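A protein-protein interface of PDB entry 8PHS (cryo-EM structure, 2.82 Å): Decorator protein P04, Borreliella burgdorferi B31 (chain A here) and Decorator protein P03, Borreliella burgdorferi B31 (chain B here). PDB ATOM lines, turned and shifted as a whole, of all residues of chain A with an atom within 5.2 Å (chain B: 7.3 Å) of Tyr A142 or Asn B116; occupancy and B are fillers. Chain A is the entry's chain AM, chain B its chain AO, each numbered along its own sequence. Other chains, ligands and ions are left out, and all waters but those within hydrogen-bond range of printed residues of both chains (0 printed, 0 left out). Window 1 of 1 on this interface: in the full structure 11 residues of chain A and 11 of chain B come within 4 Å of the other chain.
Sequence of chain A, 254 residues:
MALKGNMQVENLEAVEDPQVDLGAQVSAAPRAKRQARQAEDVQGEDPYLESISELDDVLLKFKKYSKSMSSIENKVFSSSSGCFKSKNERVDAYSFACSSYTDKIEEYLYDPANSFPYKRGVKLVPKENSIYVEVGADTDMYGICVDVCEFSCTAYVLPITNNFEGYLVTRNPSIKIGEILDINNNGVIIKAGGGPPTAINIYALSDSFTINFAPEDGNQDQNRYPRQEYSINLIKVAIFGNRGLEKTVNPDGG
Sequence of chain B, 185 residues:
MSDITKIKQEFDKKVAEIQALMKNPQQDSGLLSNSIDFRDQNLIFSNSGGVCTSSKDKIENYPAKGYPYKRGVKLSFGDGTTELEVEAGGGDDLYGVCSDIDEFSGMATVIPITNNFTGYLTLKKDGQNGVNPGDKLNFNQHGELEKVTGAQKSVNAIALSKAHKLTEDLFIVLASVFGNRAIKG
Of the 16 printed residues of chain A, 7 touch a printed residue of chain B. Hydrophobic or aromatic side chains of chain A that line the printed part of chain B: Tyr A142, Pro A159 and Ile A160. Hydrophobic or aromatic side chains of chain B that line the printed part of chain A: Phe B178.
Tyr A142 touches two residues of chain B. Printed residues of chain A within 4 Å of Asn B116: Lys A104, Glu A106, Tyr A142, Pro A159 and Thr A161. Of the printed residues of chain B, Pro A159 touches Asn B116. Printed residues of chain B within 4 Å of Glu A106: Asn B116 (2.7 Å). Of the printed residues of chain A, Ser B54 touches Lys A104. Printed residues of chain A within 4 Å of Thr B114: Thr A161 (3.3 Å). Printed residues of chain B within 4 Å of Ile A160: Phe B178 (3.8 Å). Asn B115 touches none of the printed residues of chain A. Ile B113 touches none of the printed residues of chain A. The nearest residue of chain B that does not touch Tyr A142 is Ser B176 (4.1 Å). The nearest printed residue of chain A that does not touch Asn B116 is Tyr A108 (6.0 Å). The nearest printed residue of chain A that does not touch Gly B179 is Ile A160 (5.9 Å).
OD1 of Asp B57 lies within hydrogen-bond range of ND2 of Asn B115 (2.8 Å). The side-chain carboxylate (OE1) of Glu A106 sits at hydrogen-bond distance from the side-chain hydroxyl (OH) of Tyr A108, at 2.9 Å. OE1 of Glu A106 is in hydrogen-bond range of OH of Tyr A142 (2.6 Å). N of Val A157 is in hydrogen-bond range of O of Glu A106, 2.9 Å away. The backbone carbonyl oxygen (O) of Val A122 is in hydrogen-bond range of the backbone NH (N) of Tyr A142, 2.9 Å away. The backbone NH (N) of Ile A160 is in hydrogen-bond range of the backbone carbonyl oxygen (O) of Tyr A142, 3.0 Å away.
Among the printed residues, merely in contact across the chains: Lys A104 with Ser B54, Met A141 with Phe B178, Tyr A142 with Asn B116, Tyr A142 with Phe B178, Pro A159 with Asn B116, Ile A160 with Phe B178, Thr A161 with Thr B114, Thr A161 with Asn B116, Thr A161 with Phe B178 and Thr A161 with Gly B179.
The side-chain amino group (NZ) of Lys A104 lies within salt-bridge range of the side-chain carboxylate (OD1) of Asp B57 (3.3 Å). The side-chain amide oxygen (OD1) of Asn B116 lies close to the side-chain amino group (NZ) of Lys A104, 3.3 Å away. The side-chain amide nitrogen (ND2) of Asn B116 sits at hydrogen-bond distance from the side-chain carboxylate (OE2) of Glu A106 (2.7 Å).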
ATOM      1  N   LYS A 104      29.798  24.884  -0.843  1.00  0.00           N
ATOM      2  CA  LYS A 104      30.814  23.845  -0.746  1.00  0.00           C
ATOM      3  C   LYS A 104      31.129  23.293  -2.130  1.00  0.00           C
ATOM      4  O   LYS A 104      30.225  22.881  -2.862  1.00  0.00           O
ATOM      5  CB  LYS A 104      30.343  22.725   0.181  1.00  0.00           C
ATOM      6  CG  LYS A 104      31.357  21.620   0.401  1.00  0.00           C
ATOM      7  CD  LYS A 104      31.007  20.807   1.635  1.00  0.00           C
ATOM      8  CE  LYS A 104      31.976  19.653   1.836  1.00  0.00           C
ATOM      9  NZ  LYS A 104      31.705  18.919   3.102  1.00  0.00           N
ATOM     10  N   GLU A 106      33.772  20.560  -4.162  1.00  0.00           N
ATOM     11  CA  GLU A 106      34.650  19.419  -3.955  1.00  0.00           C
ATOM     12  C   GLU A 106      35.358  19.062  -5.255  1.00  0.00           C
ATOM     13  O   GLU A 106      34.881  19.366  -6.349  1.00  0.00           O
ATOM     14  CB  GLU A 106      33.866  18.207  -3.440  1.00  0.00           C
ATOM     15  CG  GLU A 106      33.374  18.350  -2.012  1.00  0.00           C
ATOM     16  CD  GLU A 106      32.491  17.199  -1.581  1.00  0.00           C
ATOM     17  OE1 GLU A 106      32.136  16.367  -2.442  1.00  0.00           O
ATOM     18  OE2 GLU A 106      32.152  17.123  -0.382  1.00  0.00           O
ATOM     19  N   TYR A 108      37.135  15.970  -7.617  1.00  0.00           N
ATOM     20  CA  TYR A 108      37.171  14.539  -7.868  1.00  0.00           C
ATOM     21  C   TYR A 108      37.836  14.291  -9.212  1.00  0.00           C
ATOM     22  O   TYR A 108      38.043  15.209 -10.007  1.00  0.00           O
ATOM     23  CB  TYR A 108      35.769  13.926  -7.835  1.00  0.00           C
ATOM     24  CG  TYR A 108      35.146  13.895  -6.459  1.00  0.00           C
ATOM     25  CD1 TYR A 108      35.721  13.159  -5.433  1.00  0.00           C
ATOM     26  CD2 TYR A 108      33.985  14.603  -6.186  1.00  0.00           C
ATOM     27  CE1 TYR A 108      35.159  13.129  -4.174  1.00  0.00           C
ATOM     28  CE2 TYR A 108      33.414  14.577  -4.929  1.00  0.00           C
ATOM     29  CZ  TYR A 108      34.005  13.838  -3.928  1.00  0.00           C
ATOM     30  OH  TYR A 108      33.441  13.809  -2.674  1.00  0.00           O
ATOM     31  N   VAL A 122      26.467  14.389 -11.818  1.00  0.00           N
ATOM     32  CA  VAL A 122      27.467  13.340 -11.678  1.00  0.00           C
ATOM     33  C   VAL A 122      27.176  12.511 -10.434  1.00  0.00           C
ATOM     34  O   VAL A 122      26.483  12.940  -9.508  1.00  0.00           O
ATOM     35  CB  VAL A 122      28.898  13.910 -11.620  1.00  0.00           C
ATOM     36  CG1 VAL A 122      29.274  14.529 -12.956  1.00  0.00           C
ATOM     37  CG2 VAL A 122      29.021  14.927 -10.499  1.00  0.00           C
ATOM     38  N   LYS A 123      27.719  11.299 -10.436  1.00  0.00           N
ATOM     39  CA  LYS A 123      27.610  10.346  -9.347  1.00  0.00           C
ATOM     40  C   LYS A 123      29.000   9.857  -8.969  1.00  0.00           C
ATOM     41  O   LYS A 123      29.917   9.833  -9.800  1.00  0.00           O
ATOM     42  CB  LYS A 123      26.734   9.151  -9.734  1.00  0.00           C
ATOM     43  CG  LYS A 123      27.292   8.323 -10.878  1.00  0.00           C
ATOM     44  CD  LYS A 123      26.335   7.220 -11.287  1.00  0.00           C
ATOM     45  CE  LYS A 123      26.927   6.373 -12.400  1.00  0.00           C
ATOM     46  NZ  LYS A 123      25.939   5.408 -12.953  1.00  0.00           N
ATOM     47  N   LEU A 124      29.139   9.460  -7.706  1.00  0.00           N
ATOM     48  CA  LEU A 124      30.405   8.961  -7.185  1.00  0.00           C
ATOM     49  C   LEU A 124      30.546   7.478  -7.502  1.00  0.00           C
ATOM     50  O   LEU A 124      29.678   6.674  -7.145  1.00  0.00           O
ATOM     51  CB  LEU A 124      30.490   9.192  -5.678  1.00  0.00           C
ATOM     52  CG  LEU A 124      30.680  10.626  -5.186  1.00  0.00           C
ATOM     53  CD1 LEU A 124      30.572  10.676  -3.673  1.00  0.00           C
ATOM     54  CD2 LEU A 124      32.018  11.175  -5.646  1.00  0.00           C
ATOM     55  N   ASP A 140      20.609   8.383  -8.481  1.00  0.00           N
ATOM     56  CA  ASP A 140      21.874   8.177  -7.785  1.00  0.00           C
ATOM     57  C   ASP A 140      22.813   9.350  -8.011  1.00  0.00           C
ATOM     58  O   ASP A 140      24.008   9.173  -8.259  1.00  0.00           O
ATOM     59  CB  ASP A 140      22.532   6.872  -8.229  1.00  0.00           C
ATOM     60  CG  ASP A 140      22.593   6.739  -9.737  1.00  0.00           C
ATOM     61  OD1 ASP A 140      22.005   7.591 -10.435  1.00  0.00           O
ATOM     62  OD2 ASP A 140      23.234   5.785 -10.225  1.00  0.00           O
ATOM     63  N   MET A 141      22.291  10.570  -7.920  1.00  0.00           N
ATOM     64  CA  MET A 141      23.079  11.765  -8.190  1.00  0.00           C
ATOM     65  C   MET A 141      23.763  12.248  -6.919  1.00  0.00           C
ATOM     66  O   MET A 141      23.121  12.382  -5.872  1.00  0.00           O
ATOM     67  CB  MET A 141      22.200  12.875  -8.761  1.00  0.00           C
ATOM     68  CG  MET A 141      22.990  14.029  -9.344  1.00  0.00           C
ATOM     69  SD  MET A 141      21.935  15.356  -9.944  1.00  0.00           S
ATOM     70  CE  MET A 141      22.102  16.553  -8.624  1.00  0.00           C
ATOM     71  N   TYR A 142      25.066  12.504  -7.014  1.00  0.00           N
ATOM     72  CA  TYR A 142      25.808  13.087  -5.905  1.00  0.00           C
ATOM     73  C   TYR A 142      25.835  14.607  -5.952  1.00  0.00           C
ATOM     74  O   TYR A 142      25.860  15.252  -4.898  1.00  0.00           O
ATOM     75  CB  TYR A 142      27.243  12.555  -5.889  1.00  0.00           C
ATOM     76  CG  TYR A 142      28.076  13.110  -4.760  1.00  0.00           C
ATOM     77  CD1 TYR A 142      27.750  12.845  -3.438  1.00  0.00           C
ATOM     78  CD2 TYR A 142      29.187  13.902  -5.014  1.00  0.00           C
ATOM     79  CE1 TYR A 142      28.507  13.350  -2.401  1.00  0.00           C
ATOM     80  CE2 TYR A 142      29.950  14.411  -3.982  1.00  0.00           C
ATOM     81  CZ  TYR A 142      29.606  14.132  -2.678  1.00  0.00           C
ATOM     82  OH  TYR A 142      30.361  14.636  -1.645  1.00  0.00           O
ATOM     83  N   GLY A 143      25.827  15.190  -7.143  1.00  0.00           N
ATOM     84  CA  GLY A 143      25.880  16.633  -7.256  1.00  0.00           C
ATOM     85  C   GLY A 143      25.931  17.065  -8.702  1.00  0.00           C
ATOM     86  O   GLY A 143      25.584  16.303  -9.606  1.00  0.00           O
ATOM     87  N   ILE A 144      26.368  18.303  -8.910  1.00  0.00           N
ATOM     88  CA  ILE A 144      26.455  18.902 -10.236  1.00  0.00           C
ATOM     89  C   ILE A 144      27.902  19.290 -10.499  1.00  0.00           C
ATOM     90  O   ILE A 144      28.526  19.965  -9.674  1.00  0.00           O
ATOM     91  CB  ILE A 144      25.534  20.129 -10.367  1.00  0.00           C
ATOM     92  CG1 ILE A 144      24.073  19.721 -10.185  1.00  0.00           C
ATOM     93  CG2 ILE A 144      25.735  20.807 -11.709  1.00  0.00           C
ATOM     94  CD1 ILE A 144      23.558  18.810 -11.273  1.00  0.00           C
ATOM     95  N   VAL A 157      32.696  19.721  -8.157  1.00  0.00           N
ATOM     96  CA  VAL A 157      31.331  19.271  -7.924  1.00  0.00           C
ATOM     97  C   VAL A 157      30.714  20.108  -6.813  1.00  0.00           C
ATOM     98  O   VAL A 157      31.338  20.325  -5.766  1.00  0.00           O
ATOM     99  CB  VAL A 157      31.285  17.775  -7.565  1.00  0.00           C
ATOM    100  CG1 VAL A 157      29.849  17.315  -7.382  1.00  0.00           C
ATOM    101  CG2 VAL A 157      31.980  16.950  -8.636  1.00  0.00           C
ATOM    102  N   LEU A 158      29.497  20.588  -7.058  1.00  0.00           N
ATOM    103  CA  LEU A 158      28.644  21.161  -6.035  1.00  0.00           C
ATOM    104  C   LEU A 158      27.721  20.063  -5.534  1.00  0.00           C
ATOM    105  O   LEU A 158      26.920  19.538  -6.324  1.00  0.00           O
ATOM    106  CB  LEU A 158      27.833  22.322  -6.601  1.00  0.00           C
ATOM    107  CG  LEU A 158      26.916  23.093  -5.651  1.00  0.00           C
ATOM    108  CD1 LEU A 158      27.715  23.772  -4.556  1.00  0.00           C
ATOM    109  CD2 LEU A 158      26.084  24.106  -6.419  1.00  0.00           C
ATOM    110  N   PRO A 159      27.809  19.661  -4.266  1.00  0.00           N
ATOM    111  CA  PRO A 159      26.954  18.578  -3.771  1.00  0.00           C
ATOM    112  C   PRO A 159      25.478  18.935  -3.861  1.00  0.00           C
ATOM    113  O   PRO A 159      25.091  20.103  -3.799  1.00  0.00           O
ATOM    114  CB  PRO A 159      27.399  18.419  -2.314  1.00  0.00           C
ATOM    115  CG  PRO A 159      28.816  18.866  -2.320  1.00  0.00           C
ATOM    116  CD  PRO A 159      28.876  19.998  -3.310  1.00  0.00           C
ATOM    117  N   ILE A 160      24.650  17.898  -4.014  1.00  0.00           N
ATOM    118  CA  ILE A 160      23.210  18.083  -4.131  1.00  0.00           C
ATOM    119  C   ILE A 160      22.617  18.716  -2.879  1.00  0.00           C
ATOM    120  O   ILE A 160      21.531  19.304  -2.937  1.00  0.00           O
ATOM    121  CB  ILE A 160      22.530  16.734  -4.451  1.00  0.00           C
ATOM    122  CG1 ILE A 160      21.076  16.945  -4.879  1.00  0.00           C
ATOM    123  CG2 ILE A 160      22.614  15.794  -3.258  1.00  0.00           C
ATOM    124  CD1 ILE A 160      20.441  15.723  -5.493  1.00  0.00           C
ATOM    125  N   THR A 161      23.308  18.619  -1.742  1.00  0.00           N
ATOM    126  CA  THR A 161      22.824  19.250  -0.519  1.00  0.00           C
ATOM    127  C   THR A 161      22.832  20.771  -0.603  1.00  0.00           C
ATOM    128  O   THR A 161      22.192  21.426   0.226  1.00  0.00           O
ATOM    129  CB  THR A 161      23.662  18.799   0.679  1.00  0.00           C
ATOM    130  OG1 THR A 161      25.039  19.111   0.447  1.00  0.00           O
ATOM    131  CG2 THR A 161      23.518  17.304   0.896  1.00  0.00           C
ATOM    132  N   CYS B  52      38.127  14.698   4.813  1.00  0.00           N
ATOM    133  CA  CYS B  52      38.254  15.805   3.872  1.00  0.00           C
ATOM    134  C   CYS B  52      37.153  16.801   4.207  1.00  0.00           C
ATOM    135  O   CYS B  52      35.977  16.546   3.926  1.00  0.00           O
ATOM    136  CB  CYS B  52      38.146  15.310   2.429  1.00  0.00           C
ATOM    137  SG  CYS B  52      38.495  16.540   1.154  1.00  0.00           S
ATOM    138  N   SER B  54      35.477  20.862   4.582  1.00  0.00           N
ATOM    139  CA  SER B  54      35.350  22.182   3.987  1.00  0.00           C
ATOM    140  C   SER B  54      35.264  23.244   5.074  1.00  0.00           C
ATOM    141  O   SER B  54      34.711  23.014   6.152  1.00  0.00           O
ATOM    142  CB  SER B  54      34.113  22.258   3.091  1.00  0.00           C
ATOM    143  OG  SER B  54      33.863  23.587   2.675  1.00  0.00           O
ATOM    144  N   ASP B  57      31.492  24.545   6.317  1.00  0.00           N
ATOM    145  CA  ASP B  57      30.630  23.518   6.887  1.00  0.00           C
ATOM    146  C   ASP B  57      29.941  24.052   8.134  1.00  0.00           C
ATOM    147  O   ASP B  57      30.593  24.620   9.016  1.00  0.00           O
ATOM    148  CB  ASP B  57      31.430  22.261   7.226  1.00  0.00           C
ATOM    149  CG  ASP B  57      31.614  21.348   6.031  1.00  0.00           C
ATOM    150  OD1 ASP B  57      30.647  21.174   5.261  1.00  0.00           O
ATOM    151  OD2 ASP B  57      32.724  20.799   5.865  1.00  0.00           O
ATOM    152  N   ILE B 111      26.895  17.461  12.865  1.00  0.00           N
ATOM    153  CA  ILE B 111      26.849  17.979  11.503  1.00  0.00           C
ATOM    154  C   ILE B 111      25.446  17.695  10.956  1.00  0.00           C
ATOM    155  O   ILE B 111      25.083  16.518  10.810  1.00  0.00           O
ATOM    156  CB  ILE B 111      27.930  17.346  10.619  1.00  0.00           C
ATOM    157  CG1 ILE B 111      29.314  17.643  11.197  1.00  0.00           C
ATOM    158  CG2 ILE B 111      27.822  17.858   9.196  1.00  0.00           C
ATOM    159  CD1 ILE B 111      30.451  17.077  10.387  1.00  0.00           C
ATOM    160  N   PRO B 112      24.646  18.718  10.663  1.00  0.00           N
ATOM    161  CA  PRO B 112      23.263  18.470  10.233  1.00  0.00           C
ATOM    162  C   PRO B 112      23.211  17.640   8.960  1.00  0.00           C
ATOM    163  O   PRO B 112      24.123  17.670   8.132  1.00  0.00           O
ATOM    164  CB  PRO B 112      22.708  19.879  10.000  1.00  0.00           C
ATOM    165  CG  PRO B 112      23.556  20.765  10.840  1.00  0.00           C
ATOM    166  CD  PRO B 112      24.924  20.153  10.834  1.00  0.00           C
ATOM    167  N   ILE B 113      22.122  16.880   8.820  1.00  0.00           N
ATOM    168  CA  ILE B 113      21.963  16.016   7.658  1.00  0.00           C
ATOM    169  C   ILE B 113      21.860  16.819   6.368  1.00  0.00           C
ATOM    170  O   ILE B 113      22.041  16.262   5.280  1.00  0.00           O
ATOM    171  CB  ILE B 113      20.734  15.104   7.835  1.00  0.00           C
ATOM    172  CG1 ILE B 113      20.888  13.833   6.997  1.00  0.00           C
ATOM    173  CG2 ILE B 113      19.460  15.841   7.457  1.00  0.00           C
ATOM    174  CD1 ILE B 113      22.144  13.056   7.304  1.00  0.00           C
ATOM    175  N   THR B 114      21.579  18.119   6.458  1.00  0.00           N
ATOM    176  CA  THR B 114      21.557  18.974   5.280  1.00  0.00           C
ATOM    177  C   THR B 114      22.951  19.357   4.805  1.00  0.00           C
ATOM    178  O   THR B 114      23.081  19.930   3.720  1.00  0.00           O
ATOM    179  CB  THR B 114      20.750  20.243   5.565  1.00  0.00           C
ATOM    180  OG1 THR B 114      21.292  20.906   6.714  1.00  0.00           O
ATOM    181  CG2 THR B 114      19.296  19.898   5.826  1.00  0.00           C
ATOM    182  N   ASN B 115      23.985  19.058   5.585  1.00  0.00           N
ATOM    183  CA  ASN B 115      25.368  19.335   5.218  1.00  0.00           C
ATOM    184  C   ASN B 115      26.082  18.006   5.005  1.00  0.00           C
ATOM    185  O   ASN B 115      26.112  17.165   5.909  1.00  0.00           O
ATOM    186  CB  ASN B 115      26.064  20.160   6.299  1.00  0.00           C
ATOM    187  CG  ASN B 115      27.364  20.769   5.820  1.00  0.00           C
ATOM    188  OD1 ASN B 115      27.508  21.104   4.645  1.00  0.00           O
ATOM    189  ND2 ASN B 115      28.319  20.918   6.729  1.00  0.00           N
ATOM    190  N   ASN B 116      26.651  17.823   3.817  1.00  0.00           N
ATOM    191  CA  ASN B 116      27.285  16.557   3.480  1.00  0.00           C
ATOM    192  C   ASN B 116      28.539  16.334   4.319  1.00  0.00           C
ATOM    193  O   ASN B 116      29.218  17.278   4.731  1.00  0.00           O
ATOM    194  CB  ASN B 116      27.627  16.511   1.991  1.00  0.00           C
ATOM    195  CG  ASN B 116      28.757  17.446   1.623  1.00  0.00           C
ATOM    196  OD1 ASN B 116      28.691  18.646   1.879  1.00  0.00           O
ATOM    197  ND2 ASN B 116      29.803  16.899   1.014  1.00  0.00           N
ATOM    198  N   PHE B 117      28.838  15.062   4.571  1.00  0.00           N
ATOM    199  CA  PHE B 117      29.940  14.672   5.438  1.00  0.00           C
ATOM    200  C   PHE B 117      30.640  13.457   4.849  1.00  0.00           C
ATOM    201  O   PHE B 117      30.011  12.611   4.208  1.00  0.00           O
ATOM    202  CB  PHE B 117      29.442  14.365   6.859  1.00  0.00           C
ATOM    203  CG  PHE B 117      30.479  13.745   7.750  1.00  0.00           C
ATOM    204  CD1 PHE B 117      31.533  14.498   8.237  1.00  0.00           C
ATOM    205  CD2 PHE B 117      30.400  12.408   8.101  1.00  0.00           C
ATOM    206  CE1 PHE B 117      32.487  13.930   9.060  1.00  0.00           C
ATOM    207  CE2 PHE B 117      31.351  11.835   8.921  1.00  0.00           C
ATOM    208  CZ  PHE B 117      32.397  12.598   9.401  1.00  0.00           C
ATOM    209  N   THR B 118      31.951  13.382   5.069  1.00  0.00           N
ATOM    210  CA  THR B 118      32.759  12.256   4.616  1.00  0.00           C
ATOM    211  C   THR B 118      33.764  11.921   5.706  1.00  0.00           C
ATOM    212  O   THR B 118      34.609  12.754   6.044  1.00  0.00           O
ATOM    213  CB  THR B 118      33.481  12.577   3.305  1.00  0.00           C
ATOM    214  OG1 THR B 118      32.523  12.959   2.310  1.00  0.00           O
ATOM    215  CG2 THR B 118      34.254  11.364   2.814  1.00  0.00           C
ATOM    216  N   ILE B 158      26.993   6.223   1.197  1.00  0.00           N
ATOM    217  CA  ILE B 158      27.727   5.308   0.331  1.00  0.00           C
ATOM    218  C   ILE B 158      29.049   4.961   0.999  1.00  0.00           C
ATOM    219  O   ILE B 158      29.784   5.856   1.430  1.00  0.00           O
ATOM    220  CB  ILE B 158      27.967   5.913  -1.064  1.00  0.00           C
ATOM    221  CG1 ILE B 158      26.663   5.945  -1.863  1.00  0.00           C
ATOM    222  CG2 ILE B 158      29.026   5.129  -1.817  1.00  0.00           C
ATOM    223  CD1 ILE B 158      26.821   6.494  -3.262  1.00  0.00           C
ATOM    224  N   SER B 176      30.424   8.419   3.008  1.00  0.00           N
ATOM    225  CA  SER B 176      30.081   9.761   2.550  1.00  0.00           C
ATOM    226  C   SER B 176      28.564   9.896   2.579  1.00  0.00           C
ATOM    227  O   SER B 176      27.865   9.235   1.805  1.00  0.00           O
ATOM    228  CB  SER B 176      30.627  10.020   1.146  1.00  0.00           C
ATOM    229  OG  SER B 176      30.197  11.276   0.651  1.00  0.00           O
ATOM    230  N   VAL B 177      28.060  10.743   3.471  1.00  0.00           N
ATOM    231  CA  VAL B 177      26.632  11.012   3.589  1.00  0.00           C
ATOM    232  C   VAL B 177      26.341  12.332   2.891  1.00  0.00           C
ATOM    233  O   VAL B 177      26.999  13.343   3.163  1.00  0.00           O
ATOM    234  CB  VAL B 177      26.191  11.057   5.060  1.00  0.00           C
ATOM    235  CG1 VAL B 177      24.681  11.182   5.156  1.00  0.00           C
ATOM    236  CG2 VAL B 177      26.678   9.821   5.795  1.00  0.00           C
ATOM    237  N   PHE B 178      25.364  12.326   1.988  1.00  0.00           N
ATOM    238  CA  PHE B 178      25.048  13.500   1.181  1.00  0.00           C
ATOM    239  C   PHE B 178      23.541  13.727   1.111  1.00  0.00           C
ATOM    240  O   PHE B 178      22.964  13.955   0.047  1.00  0.00           O
ATOM    241  CB  PHE B 178      25.692  13.385  -0.201  1.00  0.00           C
ATOM    242  CG  PHE B 178      25.308  12.148  -0.970  1.00  0.00           C
ATOM    243  CD1 PHE B 178      26.002  10.963  -0.783  1.00  0.00           C
ATOM    244  CD2 PHE B 178      24.302  12.182  -1.920  1.00  0.00           C
ATOM    245  CE1 PHE B 178      25.673   9.830  -1.497  1.00  0.00           C
ATOM    246  CE2 PHE B 178      23.969  11.051  -2.639  1.00  0.00           C
ATOM    247  CZ  PHE B 178      24.656   9.874  -2.428  1.00  0.00           C
ATOM    248  N   GLY B 179      22.886  13.689   2.264  1.00  0.00           N
ATOM    249  CA  GLY B 179      21.522  14.160   2.381  1.00  0.00           C
ATOM    250  C   GLY B 179      20.491  13.056   2.497  1.00  0.00           C
ATOM    251  O   GLY B 179      20.769  11.925   2.900  1.00  0.00           O
